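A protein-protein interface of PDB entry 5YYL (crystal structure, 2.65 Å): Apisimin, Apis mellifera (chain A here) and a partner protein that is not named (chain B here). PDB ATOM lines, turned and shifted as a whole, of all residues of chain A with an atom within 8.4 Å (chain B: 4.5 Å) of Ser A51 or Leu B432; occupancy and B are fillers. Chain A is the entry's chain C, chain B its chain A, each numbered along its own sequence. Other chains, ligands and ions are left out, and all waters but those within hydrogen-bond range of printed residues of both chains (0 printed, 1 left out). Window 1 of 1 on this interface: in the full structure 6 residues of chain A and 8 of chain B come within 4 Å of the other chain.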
ATOM      1  N   ASN A  43      -5.364  -3.384 -19.948  1.00  0.00           N
ATOM      2  CA  ASN A  43      -4.364  -2.475 -20.498  1.00  0.00           C
ATOM      3  C   ASN A  43      -3.729  -3.062 -21.737  1.00  0.00           C
ATOM      4  O   ASN A  43      -3.628  -2.396 -22.759  1.00  0.00           O
ATOM      5  CB  ASN A  43      -3.274  -2.165 -19.475  1.00  0.00           C
ATOM      6  CG  ASN A  43      -3.768  -1.304 -18.324  1.00  0.00           C
ATOM      7  OD1 ASN A  43      -4.926  -0.865 -18.297  1.00  0.00           O
ATOM      8  ND2 ASN A  43      -2.898  -1.081 -17.348  1.00  0.00           N
ATOM      9  N   SER A  44      -3.319  -4.321 -21.644  1.00  0.00           N
ATOM     10  CA  SER A  44      -2.678  -5.020 -22.761  1.00  0.00           C
ATOM     11  C   SER A  44      -3.592  -5.120 -23.976  1.00  0.00           C
ATOM     12  O   SER A  44      -3.174  -4.851 -25.098  1.00  0.00           O
ATOM     13  CB  SER A  44      -2.231  -6.416 -22.315  1.00  0.00           C
ATOM     14  OG  SER A  44      -1.723  -7.172 -23.392  1.00  0.00           O
ATOM     15  N   LEU A  45      -4.841  -5.484 -23.732  1.00  0.00           N
ATOM     16  CA  LEU A  45      -5.822  -5.693 -24.789  1.00  0.00           C
ATOM     17  C   LEU A  45      -6.208  -4.422 -25.543  1.00  0.00           C
ATOM     18  O   LEU A  45      -6.337  -4.422 -26.770  1.00  0.00           O
ATOM     19  CB  LEU A  45      -7.079  -6.299 -24.174  1.00  0.00           C
ATOM     20  CG  LEU A  45      -8.208  -6.666 -25.123  1.00  0.00           C
ATOM     21  CD1 LEU A  45      -7.763  -7.828 -26.005  1.00  0.00           C
ATOM     22  CD2 LEU A  45      -9.441  -7.016 -24.288  1.00  0.00           C
ATOM     23  N   VAL A  46      -6.437  -3.353 -24.787  1.00  0.00           N
ATOM     24  CA  VAL A  46      -6.869  -2.087 -25.361  1.00  0.00           C
ATOM     25  C   VAL A  46      -5.736  -1.486 -26.185  1.00  0.00           C
ATOM     26  O   VAL A  46      -5.968  -0.941 -27.291  1.00  0.00           O
ATOM     27  CB  VAL A  46      -7.344  -1.124 -24.263  1.00  0.00           C
ATOM     28  CG1 VAL A  46      -7.564   0.283 -24.807  1.00  0.00           C
ATOM     29  CG2 VAL A  46      -8.633  -1.681 -23.651  1.00  0.00           C
ATOM     30  N   SER A  47      -4.520  -1.610 -25.642  1.00  0.00           N
ATOM     31  CA  SER A  47      -3.307  -1.205 -26.350  1.00  0.00           C
ATOM     32  C   SER A  47      -3.206  -1.898 -27.698  1.00  0.00           C
ATOM     33  O   SER A  47      -2.949  -1.234 -28.685  1.00  0.00           O
ATOM     34  CB  SER A  47      -2.048  -1.478 -25.510  1.00  0.00           C
ATOM     35  OG  SER A  47      -1.193  -0.348 -25.500  1.00  0.00           O
ATOM     36  N   SER A  48      -3.442  -3.216 -27.745  1.00  0.00           N
ATOM     37  CA  SER A  48      -3.508  -3.942 -29.026  1.00  0.00           C
ATOM     38  C   SER A  48      -4.505  -3.319 -29.963  1.00  0.00           C
ATOM     39  O   SER A  48      -4.143  -2.990 -31.096  1.00  0.00           O
ATOM     40  CB  SER A  48      -3.916  -5.409 -28.852  1.00  0.00           C
ATOM     41  OG  SER A  48      -2.933  -6.119 -28.156  1.00  0.00           O
ATOM     42  N   ILE A  49      -5.749  -3.153 -29.482  1.00  0.00           N
ATOM     43  CA  ILE A  49      -6.855  -2.669 -30.321  1.00  0.00           C
ATOM     44  C   ILE A  49      -6.511  -1.292 -30.869  1.00  0.00           C
ATOM     45  O   ILE A  49      -6.551  -1.084 -32.079  1.00  0.00           O
ATOM     46  CB  ILE A  49      -8.223  -2.602 -29.579  1.00  0.00           C
ATOM     47  CG1 ILE A  49      -8.677  -3.981 -29.109  1.00  0.00           C
ATOM     48  CG2 ILE A  49      -9.316  -2.026 -30.483  1.00  0.00           C
ATOM     49  CD1 ILE A  49      -9.619  -3.909 -27.923  1.00  0.00           C
ATOM     50  N   VAL A  50      -6.144  -0.366 -29.989  1.00  0.00           N
ATOM     51  CA  VAL A  50      -5.882   0.994 -30.457  1.00  0.00           C
ATOM     52  C   VAL A  50      -4.641   1.098 -31.338  1.00  0.00           C
ATOM     53  O   VAL A  50      -4.560   2.008 -32.159  1.00  0.00           O
ATOM     54  CB  VAL A  50      -5.857   2.053 -29.314  1.00  0.00           C
ATOM     55  CG1 VAL A  50      -7.184   2.050 -28.582  1.00  0.00           C
ATOM     56  CG2 VAL A  50      -4.687   1.853 -28.360  1.00  0.00           C
ATOM     57  N   SER A  51      -3.691   0.176 -31.185  1.00  0.00           N
ATOM     58  CA  SER A  51      -2.459   0.202 -31.992  1.00  0.00           C
ATOM     59  C   SER A  51      -2.664  -0.260 -33.436  1.00  0.00           C
ATOM     60  O   SER A  51      -1.769  -0.090 -34.242  1.00  0.00           O
ATOM     61  CB  SER A  51      -1.359  -0.650 -31.359  1.00  0.00           C
ATOM     62  OG  SER A  51      -1.597  -2.041 -31.553  1.00  0.00           O
ATOM     63  N   GLY A  52      -3.802  -0.883 -33.743  1.00  0.00           N
ATOM     64  CA  GLY A  52      -4.049  -1.428 -35.073  1.00  0.00           C
ATOM     65  C   GLY A  52      -3.624  -2.880 -35.226  1.00  0.00           C
ATOM     66  O   GLY A  52      -3.892  -3.509 -36.251  1.00  0.00           O
ATOM     67  N   ALA A  53      -2.976  -3.419 -34.197  1.00  0.00           N
ATOM     68  CA  ALA A  53      -2.569  -4.816 -34.179  1.00  0.00           C
ATOM     69  C   ALA A  53      -3.753  -5.793 -34.266  1.00  0.00           C
ATOM     70  O   ALA A  53      -4.893  -5.430 -33.987  1.00  0.00           O
ATOM     71  CB  ALA A  53      -1.767  -5.101 -32.918  1.00  0.00           C
ATOM     72  N   ASN A  54      -3.469  -7.024 -34.696  1.00  0.00           N
ATOM     73  CA  ASN A  54      -4.419  -8.139 -34.569  1.00  0.00           C
ATOM     74  C   ASN A  54      -4.486  -8.450 -33.084  1.00  0.00           C
ATOM     75  O   ASN A  54      -3.464  -8.381 -32.389  1.00  0.00           O
ATOM     76  CB  ASN A  54      -3.979  -9.395 -35.359  1.00  0.00           C
ATOM     77  CG  ASN A  54      -4.065  -9.214 -36.879  1.00  0.00           C
ATOM     78  OD1 ASN A  54      -4.785  -8.342 -37.392  1.00  0.00           O
ATOM     79  ND2 ASN A  54      -3.331 -10.060 -37.611  1.00  0.00           N
ATOM     80  N   VAL A  55      -5.677  -8.795 -32.605  1.00  0.00           N
ATOM     81  CA  VAL A  55      -5.931  -8.908 -31.165  1.00  0.00           C
ATOM     82  C   VAL A  55      -6.306 -10.345 -30.784  1.00  0.00           C
ATOM     83  O   VAL A  55      -7.162 -10.958 -31.411  1.00  0.00           O
ATOM     84  CB  VAL A  55      -6.984  -7.868 -30.688  1.00  0.00           C
ATOM     85  CG1 VAL A  55      -8.125  -7.718 -31.685  1.00  0.00           C
ATOM     86  CG2 VAL A  55      -7.522  -8.213 -29.293  1.00  0.00           C
ATOM     87  N   LEU B  34       6.454   3.783 -22.244  1.00  0.00           N
ATOM     88  CA  LEU B  34       6.011   2.635 -23.017  1.00  0.00           C
ATOM     89  C   LEU B  34       7.126   1.580 -23.054  1.00  0.00           C
ATOM     90  O   LEU B  34       6.847   0.392 -22.963  1.00  0.00           O
ATOM     91  CB  LEU B  34       5.668   3.103 -24.423  1.00  0.00           C
ATOM     92  CG  LEU B  34       4.949   2.154 -25.358  1.00  0.00           C
ATOM     93  CD1 LEU B  34       3.570   1.821 -24.850  1.00  0.00           C
ATOM     94  CD2 LEU B  34       4.852   2.721 -26.757  1.00  0.00           C
ATOM     95  N   GLN B  71       5.913   3.584 -35.390  1.00  0.00           N
ATOM     96  CA  GLN B  71       4.949   2.614 -34.914  1.00  0.00           C
ATOM     97  C   GLN B  71       3.984   2.311 -36.028  1.00  0.00           C
ATOM     98  O   GLN B  71       3.490   3.238 -36.673  1.00  0.00           O
ATOM     99  CB  GLN B  71       4.209   3.191 -33.705  1.00  0.00           C
ATOM    100  CG  GLN B  71       3.112   2.306 -33.122  1.00  0.00           C
ATOM    101  CD  GLN B  71       1.780   2.380 -33.855  1.00  0.00           C
ATOM    102  OE1 GLN B  71       1.391   3.436 -34.349  1.00  0.00           O
ATOM    103  NE2 GLN B  71       1.079   1.260 -33.931  1.00  0.00           N
ATOM    104  N   HIS B  73       0.834  -0.823 -36.452  1.00  0.00           N
ATOM    105  CA  HIS B  73       0.180  -2.004 -35.881  1.00  0.00           C
ATOM    106  C   HIS B  73       0.957  -2.474 -34.637  1.00  0.00           C
ATOM    107  O   HIS B  73       1.193  -1.668 -33.742  1.00  0.00           O
ATOM    108  CB  HIS B  73       0.003  -3.087 -36.953  1.00  0.00           C
ATOM    109  CG  HIS B  73      -0.931  -2.706 -38.061  1.00  0.00           C
ATOM    110  ND1 HIS B  73      -1.311  -3.597 -39.044  1.00  0.00           N
ATOM    111  CD2 HIS B  73      -1.585  -1.549 -38.331  1.00  0.00           C
ATOM    112  CE1 HIS B  73      -2.148  -2.999 -39.877  1.00  0.00           C
ATOM    113  NE2 HIS B  73      -2.329  -1.753 -39.470  1.00  0.00           N
ATOM    114  N   ILE B  76       6.911  -1.564 -33.190  1.00  0.00           N
ATOM    115  CA  ILE B  76       7.515  -0.306 -32.780  1.00  0.00           C
ATOM    116  C   ILE B  76       8.908  -0.317 -33.396  1.00  0.00           C
ATOM    117  O   ILE B  76       9.730  -1.138 -33.011  1.00  0.00           O
ATOM    118  CB  ILE B  76       7.665  -0.214 -31.237  1.00  0.00           C
ATOM    119  CG1 ILE B  76       6.309  -0.197 -30.524  1.00  0.00           C
ATOM    120  CG2 ILE B  76       8.490   1.004 -30.835  1.00  0.00           C
ATOM    121  CD1 ILE B  76       5.501   1.073 -30.687  1.00  0.00           C
ATOM    122  N   LEU B 363      -6.808   3.369 -33.562  1.00  0.00           N
ATOM    123  CA  LEU B 363      -7.418   2.533 -34.604  1.00  0.00           C
ATOM    124  C   LEU B 363      -8.301   1.475 -33.942  1.00  0.00           C
ATOM    125  O   LEU B 363      -8.158   1.233 -32.745  1.00  0.00           O
ATOM    126  CB  LEU B 363      -6.325   1.841 -35.441  1.00  0.00           C
ATOM    127  CG  LEU B 363      -5.507   2.671 -36.455  1.00  0.00           C
ATOM    128  CD1 LEU B 363      -4.264   1.910 -36.891  1.00  0.00           C
ATOM    129  CD2 LEU B 363      -6.372   3.023 -37.658  1.00  0.00           C
ATOM    130  N   TYR B 377      -2.454  10.477 -30.313  1.00  0.00           N
ATOM    131  CA  TYR B 377      -1.462  10.330 -29.249  1.00  0.00           C
ATOM    132  C   TYR B 377      -0.054  10.503 -29.785  1.00  0.00           C
ATOM    133  O   TYR B 377       0.208  10.268 -30.968  1.00  0.00           O
ATOM    134  CB  TYR B 377      -1.588   8.962 -28.560  1.00  0.00           C
ATOM    135  CG  TYR B 377      -1.409   7.748 -29.444  1.00  0.00           C
ATOM    136  CD1 TYR B 377      -2.464   7.234 -30.193  1.00  0.00           C
ATOM    137  CD2 TYR B 377      -0.186   7.077 -29.496  1.00  0.00           C
ATOM    138  CE1 TYR B 377      -2.288   6.109 -30.988  1.00  0.00           C
ATOM    139  CE2 TYR B 377      -0.006   5.934 -30.286  1.00  0.00           C
ATOM    140  CZ  TYR B 377      -1.047   5.462 -31.032  1.00  0.00           C
ATOM    141  OH  TYR B 377      -0.864   4.351 -31.826  1.00  0.00           O
ATOM    142  N   LEU B 379       4.185   9.787 -29.479  1.00  0.00           N
ATOM    143  CA  LEU B 379       5.287   8.923 -29.053  1.00  0.00           C
ATOM    144  C   LEU B 379       6.563   9.755 -29.019  1.00  0.00           C
ATOM    145  O   LEU B 379       6.881  10.439 -29.979  1.00  0.00           O
ATOM    146  CB  LEU B 379       5.475   7.788 -30.067  1.00  0.00           C
ATOM    147  CG  LEU B 379       4.297   6.842 -30.321  1.00  0.00           C
ATOM    148  CD1 LEU B 379       4.520   6.020 -31.574  1.00  0.00           C
ATOM    149  CD2 LEU B 379       4.064   5.969 -29.104  1.00  0.00           C
ATOM    150  N   ASN B 404       4.837   8.216 -24.103  1.00  0.00           N
ATOM    151  CA  ASN B 404       3.657   8.516 -24.899  1.00  0.00           C
ATOM    152  C   ASN B 404       2.608   9.218 -24.076  1.00  0.00           C
ATOM    153  O   ASN B 404       2.735   9.319 -22.860  1.00  0.00           O
ATOM    154  CB  ASN B 404       3.088   7.263 -25.624  1.00  0.00           C
ATOM    155  CG  ASN B 404       2.496   6.236 -24.676  1.00  0.00           C
ATOM    156  OD1 ASN B 404       2.792   6.224 -23.465  1.00  0.00           O
ATOM    157  ND2 ASN B 404       1.638   5.361 -25.217  1.00  0.00           N
ATOM    158  N   HIS B 431      -4.046   6.408 -25.505  1.00  0.00           N
ATOM    159  CA  HIS B 431      -2.676   6.202 -25.991  1.00  0.00           C
ATOM    160  C   HIS B 431      -2.337   4.704 -25.872  1.00  0.00           C
ATOM    161  O   HIS B 431      -3.239   3.897 -25.636  1.00  0.00           O
ATOM    162  CB  HIS B 431      -1.684   7.116 -25.269  1.00  0.00           C
ATOM    163  CG  HIS B 431      -1.647   6.952 -23.788  1.00  0.00           C
ATOM    164  ND1 HIS B 431      -1.271   5.777 -23.180  1.00  0.00           N
ATOM    165  CD2 HIS B 431      -1.897   7.831 -22.783  1.00  0.00           C
ATOM    166  CE1 HIS B 431      -1.294   5.936 -21.867  1.00  0.00           C
ATOM    167  NE2 HIS B 431      -1.684   7.169 -21.600  1.00  0.00           N
ATOM    168  N   LEU B 432      -1.084   4.313 -26.084  1.00  0.00           N
ATOM    169  CA  LEU B 432      -0.688   2.896 -25.905  1.00  0.00           C
ATOM    170  C   LEU B 432      -0.353   2.532 -24.433  1.00  0.00           C
ATOM    171  O   LEU B 432      -0.052   1.376 -24.116  1.00  0.00           O
ATOM    172  CB  LEU B 432       0.479   2.527 -26.828  1.00  0.00           C
ATOM    173  CG  LEU B 432       0.379   2.852 -28.322  1.00  0.00           C
ATOM    174  CD1 LEU B 432       1.607   2.347 -29.051  1.00  0.00           C
ATOM    175  CD2 LEU B 432      -0.864   2.283 -28.989  1.00  0.00           C
ATOM    176  OXT LEU B 432      -0.378   3.357 -23.511  1.00  0.00           O
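NE2 of Gln B71 sits at hydrogen-bond distance from O of Ser A51. The backbone carbonyl oxygen (O) of Ser A51 lies close to the backbone NH (N) of His B73 (3.5 Å). The backbone carbonyl oxygen (O) of Val A50 lies within hydrogen-bond range of the backbone NH (N) of Leu B363, 3.0 Å away. The chain-end carboxylate of Leu B432 sits at hydrogen-bond distance from the side-chain hydroxyl of Ser A47 (2.5 Å). The backbone carbonyl oxygen (O) of Ile A49 lies close to the backbone carbonyl oxygen (O) of Leu B363 (2.9 Å).
The backbone carbonyl oxygen of His B73 sits at hydrogen-bond distance from the side-chain amide nitrogen of Gln B71 (2.9 Å). The backbone NH of Leu B432 sits close to the side-chain amide nitrogen of Asn B404, 3.0 Å away. O of Ser A47 lies close to OG of Ser A51 (3.3 Å). O of Ser A48 sits at hydrogen-bond distance from OG of Ser A51, at 2.8 Å. The backbone NH (N) of Ala A53 lies within hydrogen-bond range of the backbone carbonyl oxygen (O) of Ser A48 (3.3 Å). The backbone NH (N) of Ala A53 lies close to the side-chain hydroxyl (OG) of Ser A51.
Among the printed residues, merely in contact across the chains: Gly A52 with His B73 (3.6 Å), Val A50 with His B431 (3.7 Å), Ser A51 with Leu B432 (3.8 Å), Gly A52 with Leu B363 (3.8 Å), Ala A53 with His B73 (3.8 Å) and Val A50 with Leu B432 (3.9 Å).
Val A46 touches none of the printed residues of chain B. Of the printed residues of chain B, Ser A47 touches Leu B432 (2.5 Å). Of the printed residues of chain B, Val A50 touches Leu B363, His B431 and Leu B432. Ser A51 touches just these residues of chain B: Gln B71, His B73 and Leu B432. Of the printed residues of chain B, Gly A52 touches His B73 and Leu B363. Printed residues of chain A within 4 Å of His B73: Ser A51 (3.2 Å), Gly A52 (3.6 Å) and Ala A53 (3.8 Å). The nearest printed residue of chain A that does not touch Gln B71 is Gly A52 (5.3 Å).
Of the 10 printed residues of chain B, 5 touch a printed residue of chain A. Hydrophobic or aromatic side chains of chain B within 4 Å of the printed part of chain A: His B73, Leu B363 and Leu B432. Among the printed residues, 11 pairs touch across the chains.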
